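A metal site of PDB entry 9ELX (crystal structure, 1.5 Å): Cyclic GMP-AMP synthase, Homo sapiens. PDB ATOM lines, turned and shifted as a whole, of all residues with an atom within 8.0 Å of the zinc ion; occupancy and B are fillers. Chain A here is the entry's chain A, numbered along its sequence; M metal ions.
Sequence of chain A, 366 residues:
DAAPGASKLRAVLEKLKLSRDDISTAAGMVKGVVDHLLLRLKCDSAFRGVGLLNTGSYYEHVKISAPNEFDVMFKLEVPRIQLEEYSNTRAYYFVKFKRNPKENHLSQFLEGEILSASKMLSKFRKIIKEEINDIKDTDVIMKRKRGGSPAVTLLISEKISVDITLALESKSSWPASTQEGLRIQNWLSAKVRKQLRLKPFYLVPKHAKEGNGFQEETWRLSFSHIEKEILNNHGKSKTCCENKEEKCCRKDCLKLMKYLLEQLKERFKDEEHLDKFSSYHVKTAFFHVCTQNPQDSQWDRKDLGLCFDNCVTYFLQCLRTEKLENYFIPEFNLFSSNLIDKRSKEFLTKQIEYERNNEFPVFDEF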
ATOM      1  N   LEU A 231      -7.551  23.883  27.117  1.00  0.00           N
ATOM      2  CA  LEU A 231      -7.362  25.146  26.406  1.00  0.00           C
ATOM      3  C   LEU A 231      -7.171  26.310  27.376  1.00  0.00           C
ATOM      4  O   LEU A 231      -6.422  27.250  27.053  1.00  0.00           O
ATOM      5  CB  LEU A 231      -8.540  25.444  25.457  1.00  0.00           C
ATOM      6  CG  LEU A 231      -8.268  24.732  24.118  1.00  0.00           C
ATOM      7  CD1 LEU A 231      -9.505  24.687  23.269  1.00  0.00           C
ATOM      8  CD2 LEU A 231      -7.154  25.418  23.309  1.00  0.00           C
ATOM      9  N   ASN A 233      -5.791  26.207  30.276  1.00  0.00           N
ATOM     10  CA  ASN A 233      -4.656  25.972  31.176  1.00  0.00           C
ATOM     11  C   ASN A 233      -3.677  25.170  30.337  1.00  0.00           C
ATOM     12  O   ASN A 233      -3.460  23.975  30.531  1.00  0.00           O
ATOM     13  CB  ASN A 233      -5.064  25.250  32.446  1.00  0.00           C
ATOM     14  CG  ASN A 233      -4.038  25.362  33.532  1.00  0.00           C
ATOM     15  OD1 ASN A 233      -2.937  25.890  33.306  1.00  0.00           O
ATOM     16  ND2 ASN A 233      -4.368  24.806  34.715  1.00  0.00           N
ATOM     17  N   HIS A 234      -3.097  25.833  29.323  1.00  0.00           N
ATOM     18  CA  HIS A 234      -2.592  25.141  28.157  1.00  0.00           C
ATOM     19  C   HIS A 234      -1.077  25.102  28.076  1.00  0.00           C
ATOM     20  O   HIS A 234      -0.538  24.546  27.105  1.00  0.00           O
ATOM     21  CB  HIS A 234      -3.140  25.839  26.890  1.00  0.00           C
ATOM     22  CG  HIS A 234      -2.709  27.260  26.815  1.00  0.00           C
ATOM     23  ND1 HIS A 234      -3.582  28.314  26.894  1.00  0.00           N
ATOM     24  CD2 HIS A 234      -1.454  27.800  26.784  1.00  0.00           C
ATOM     25  CE1 HIS A 234      -2.900  29.454  26.842  1.00  0.00           C
ATOM     26  NE2 HIS A 234      -1.610  29.164  26.768  1.00  0.00           N
ATOM     27  N   GLY A 235      -0.379  25.665  29.045  1.00  0.00           N
ATOM     28  CA  GLY A 235       1.078  25.757  28.957  1.00  0.00           C
ATOM     29  C   GLY A 235       1.769  24.652  29.747  1.00  0.00           C
ATOM     30  O   GLY A 235       1.197  24.081  30.667  1.00  0.00           O
ATOM     31  N   LYS A 236       3.009  24.357  29.386  1.00  0.00           N
ATOM     32  CA  LYS A 236       3.871  23.594  30.292  1.00  0.00           C
ATOM     33  C   LYS A 236       4.130  24.395  31.574  1.00  0.00           C
ATOM     34  O   LYS A 236       4.036  23.862  32.687  1.00  0.00           O
ATOM     35  CB  LYS A 236       5.202  23.225  29.625  1.00  0.00           C
ATOM     36  CG  LYS A 236       6.072  22.519  30.663  1.00  0.00           C
ATOM     37  CD  LYS A 236       7.328  21.866  30.057  1.00  0.00           C
ATOM     38  CE  LYS A 236       6.947  20.722  29.114  1.00  0.00           C
ATOM     39  NZ  LYS A 236       6.218  19.725  29.914  1.00  0.00           N
ATOM     40  N   SER A 237       4.406  25.691  31.424  1.00  0.00           N
ATOM     41  CA  SER A 237       4.518  26.570  32.568  1.00  0.00           C
ATOM     42  C   SER A 237       3.123  26.915  33.103  1.00  0.00           C
ATOM     43  O   SER A 237       2.224  27.254  32.339  1.00  0.00           O
ATOM     44  CB  SER A 237       5.203  27.869  32.186  1.00  0.00           C
ATOM     45  OG  SER A 237       5.054  28.808  33.232  1.00  0.00           O
ATOM     46  N   THR A 239       2.370  29.559  34.499  1.00  0.00           N
ATOM     47  CA  THR A 239       2.078  30.957  34.261  1.00  0.00           C
ATOM     48  C   THR A 239       2.085  31.312  32.781  1.00  0.00           C
ATOM     49  O   THR A 239       2.127  32.501  32.447  1.00  0.00           O
ATOM     50  CB  THR A 239       3.042  31.866  35.032  1.00  0.00           C
ATOM     51  OG1 THR A 239       4.389  31.394  34.902  1.00  0.00           O
ATOM     52  CG2 THR A 239       2.668  31.889  36.506  1.00  0.00           C
ATOM     53  N   CYS A 240       2.010  30.312  31.880  1.00  0.00           N
ATOM     54  CA  CYS A 240       1.896  30.589  30.459  1.00  0.00           C
ATOM     55  C   CYS A 240       0.737  31.563  30.207  1.00  0.00           C
ATOM     56  O   CYS A 240      -0.371  31.360  30.701  1.00  0.00           O
ATOM     57  CB  CYS A 240       1.716  29.251  29.714  1.00  0.00           C
ATOM     58  SG  CYS A 240       1.903  29.462  27.898  1.00  0.00           S
ATOM     59  N   CYS A 241       1.044  32.630  29.488  1.00  0.00           N
ATOM     60  CA  CYS A 241       0.086  33.668  29.119  1.00  0.00           C
ATOM     61  C   CYS A 241      -0.437  34.459  30.318  1.00  0.00           C
ATOM     62  O   CYS A 241      -1.422  35.178  30.188  1.00  0.00           O
ATOM     63  CB  CYS A 241      -1.091  33.105  28.307  1.00  0.00           C
ATOM     64  SG  CYS A 241      -0.515  32.536  26.658  1.00  0.00           S
ATOM     65  N   GLU A 242       0.203  34.364  31.490  1.00  0.00           N
ATOM     66  CA  GLU A 242      -0.179  35.205  32.608  1.00  0.00           C
ATOM     67  C   GLU A 242       0.723  36.414  32.734  1.00  0.00           C
ATOM     68  O   GLU A 242       0.484  37.286  33.584  1.00  0.00           O
ATOM     69  CB  GLU A 242      -0.141  34.391  33.909  1.00  0.00           C
ATOM     70  CG  GLU A 242      -1.403  33.576  34.079  1.00  0.00           C
ATOM     71  CD  GLU A 242      -1.552  33.006  35.495  1.00  0.00           C
ATOM     72  OE1 GLU A 242      -0.692  33.324  36.392  1.00  0.00           O
ATOM     73  OE2 GLU A 242      -2.600  32.354  35.724  1.00  0.00           O
ATOM     74  N   ASN A 243       1.776  36.490  31.931  1.00  0.00           N
ATOM     75  CA  ASN A 243       2.645  37.658  31.981  1.00  0.00           C
ATOM     76  C   ASN A 243       3.255  37.885  30.599  1.00  0.00           C
ATOM     77  O   ASN A 243       3.158  37.052  29.694  1.00  0.00           O
ATOM     78  CB  ASN A 243       3.728  37.509  33.056  1.00  0.00           C
ATOM     79  CG  ASN A 243       4.652  36.307  32.809  1.00  0.00           C
ATOM     80  OD1 ASN A 243       5.517  36.356  31.929  1.00  0.00           O
ATOM     81  ND2 ASN A 243       4.482  35.231  33.594  1.00  0.00           N
ATOM     82  N   GLU A 246       5.626  35.395  28.884  1.00  0.00           N
ATOM     83  CA  GLU A 246       5.166  34.039  28.567  1.00  0.00           C
ATOM     84  C   GLU A 246       3.876  34.037  27.735  1.00  0.00           C
ATOM     85  O   GLU A 246       2.979  33.195  27.931  1.00  0.00           O
ATOM     86  CB  GLU A 246       4.940  33.240  29.852  1.00  0.00           C
ATOM     87  CG  GLU A 246       6.174  33.021  30.681  1.00  0.00           C
ATOM     88  CD  GLU A 246       5.884  32.139  31.891  1.00  0.00           C
ATOM     89  OE1 GLU A 246       5.702  30.920  31.701  1.00  0.00           O
ATOM     90  OE2 GLU A 246       5.814  32.660  33.035  1.00  0.00           O
ATOM     91  N   LYS A 247       3.775  34.922  26.748  1.00  0.00           N
ATOM     92  CA  LYS A 247       2.589  35.000  25.898  1.00  0.00           C
ATOM     93  C   LYS A 247       2.814  34.089  24.714  1.00  0.00           C
ATOM     94  O   LYS A 247       3.318  34.496  23.678  1.00  0.00           O
ATOM     95  CB  LYS A 247       2.331  36.427  25.431  1.00  0.00           C
ATOM     96  CG  LYS A 247       1.973  37.394  26.515  1.00  0.00           C
ATOM     97  CD  LYS A 247       0.616  37.052  27.115  1.00  0.00           C
ATOM     98  CE  LYS A 247       0.421  37.748  28.460  1.00  0.00           C
ATOM     99  NZ  LYS A 247      -0.995  37.789  28.882  1.00  0.00           N
ATOM    100  N   CYS A 248       2.387  32.854  24.854  1.00  0.00           N
ATOM    101  CA  CYS A 248       2.604  31.913  23.757  1.00  0.00           C
ATOM    102  C   CYS A 248       1.580  32.137  22.639  1.00  0.00           C
ATOM    103  O   CYS A 248       0.620  32.911  22.753  1.00  0.00           O
ATOM    104  CB  CYS A 248       2.528  30.461  24.279  1.00  0.00           C
ATOM    105  SG  CYS A 248       0.817  29.784  24.497  1.00  0.00           S
ATOM    106  N   CYS A 249       1.764  31.434  21.514  1.00  0.00           N
ATOM    107  CA  CYS A 249       0.837  31.617  20.404  1.00  0.00           C
ATOM    108  C   CYS A 249      -0.054  30.406  20.152  1.00  0.00           C
ATOM    109  O   CYS A 249      -0.594  30.266  19.053  1.00  0.00           O
ATOM    110  CB  CYS A 249       1.597  31.978  19.119  1.00  0.00           C
ATOM    111  SG  CYS A 249       2.729  30.680  18.457  1.00  0.00           S
ATOM    112  N   ARG A 250      -0.229  29.529  21.144  1.00  0.00           N
ATOM    113  CA  ARG A 250      -1.067  28.344  20.924  1.00  0.00           C
ATOM    114  C   ARG A 250      -2.491  28.732  20.528  1.00  0.00           C
ATOM    115  O   ARG A 250      -2.999  28.269  19.495  1.00  0.00           O
ATOM    116  CB  ARG A 250      -1.109  27.490  22.196  1.00  0.00           C
ATOM    117  CG  ARG A 250       0.161  26.678  22.431  1.00  0.00           C
ATOM    118  CD  ARG A 250      -0.062  25.760  23.689  1.00  0.00           C
ATOM    119  NE  ARG A 250       1.154  25.014  24.001  1.00  0.00           N
ATOM    120  CZ  ARG A 250       2.068  25.417  24.876  1.00  0.00           C
ATOM    121  NH1 ARG A 250       2.014  26.648  25.436  1.00  0.00           N
ATOM    122  NH2 ARG A 250       2.984  24.518  25.302  1.00  0.00           N
ATOM    123  N   LYS A 251      -3.146  29.611  21.303  1.00  0.00           N
ATOM    124  CA  LYS A 251      -4.529  29.976  21.003  1.00  0.00           C
ATOM    125  C   LYS A 251      -4.621  30.723  19.688  1.00  0.00           C
ATOM    126  O   LYS A 251      -5.588  30.522  18.942  1.00  0.00           O
ATOM    127  CB  LYS A 251      -5.168  30.794  22.120  1.00  0.00           C
ATOM    128  CG  LYS A 251      -5.561  29.890  23.267  1.00  0.00           C
ATOM    129  CD  LYS A 251      -6.567  30.606  24.188  1.00  0.00           C
ATOM    130  CE  LYS A 251      -6.798  29.606  25.294  1.00  0.00           C
ATOM    131  NZ  LYS A 251      -7.773  30.080  26.284  1.00  0.00           N
ATOM    132  N   ASP A 296       6.760  25.233  25.831  1.00  0.00           N
ATOM    133  CA  ASP A 296       6.253  26.573  25.558  1.00  0.00           C
ATOM    134  C   ASP A 296       7.177  27.278  24.576  1.00  0.00           C
ATOM    135  O   ASP A 296       6.712  28.067  23.752  1.00  0.00           O
ATOM    136  CB  ASP A 296       6.075  27.415  26.844  1.00  0.00           C
ATOM    137  CG  ASP A 296       5.100  26.801  27.834  1.00  0.00           C
ATOM    138  OD1 ASP A 296       4.205  26.083  27.399  1.00  0.00           O
ATOM    139  OD2 ASP A 296       5.224  27.113  29.025  1.00  0.00           O
ATOM    140  N   TRP A 299       6.159  27.471  20.978  1.00  0.00           N
ATOM    141  CA  TRP A 299       4.992  28.293  20.700  1.00  0.00           C
ATOM    142  C   TRP A 299       5.269  29.753  21.045  1.00  0.00           C
ATOM    143  O   TRP A 299       4.404  30.519  21.533  1.00  0.00           O
ATOM    144  CB  TRP A 299       3.812  27.759  21.501  1.00  0.00           C
ATOM    145  CG  TRP A 299       3.454  26.364  21.126  1.00  0.00           C
ATOM    146  CD1 TRP A 299       3.865  25.170  21.742  1.00  0.00           C
ATOM    147  CD2 TRP A 299       2.603  25.986  20.031  1.00  0.00           C
ATOM    148  NE1 TRP A 299       3.300  24.109  21.081  1.00  0.00           N
ATOM    149  CE2 TRP A 299       2.501  24.574  20.052  1.00  0.00           C
ATOM    150  CE3 TRP A 299       1.930  26.703  19.055  1.00  0.00           C
ATOM    151  CZ2 TRP A 299       1.753  23.853  19.134  1.00  0.00           C
ATOM    152  CZ3 TRP A 299       1.147  25.987  18.116  1.00  0.00           C
ATOM    153  CH2 TRP A 299       1.060  24.559  18.182  1.00  0.00           C
HETATM  154 ZN    ZN M   1       0.174  30.355  26.700  1.00  0.00          ZN
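The nearest printed residue that does not touch the zinc ion is Glu 246 (4.2 Å).
ND1 of His 234 lies within hydrogen-bond range of O of Leu 231 (3.0 Å). The side-chain sulfur of Cys 240 sits close to the guanidinium group of Arg 250. N of Cys 241 is in hydrogen-bond range of O of Glu 246, at 2.5 Å. NZ of Lys 247 lies within hydrogen-bond range of O of Cys 241, 3.0 Å away. The side-chain sulfur (SG) of Cys 248 sits close to the guanidinium group (NH1) of Arg 250, 3.5 Å away.
The zinc ion is bound by NE2 of His 234, SG of Cys 240, SG of Cys 241 and SG of Cys 248.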
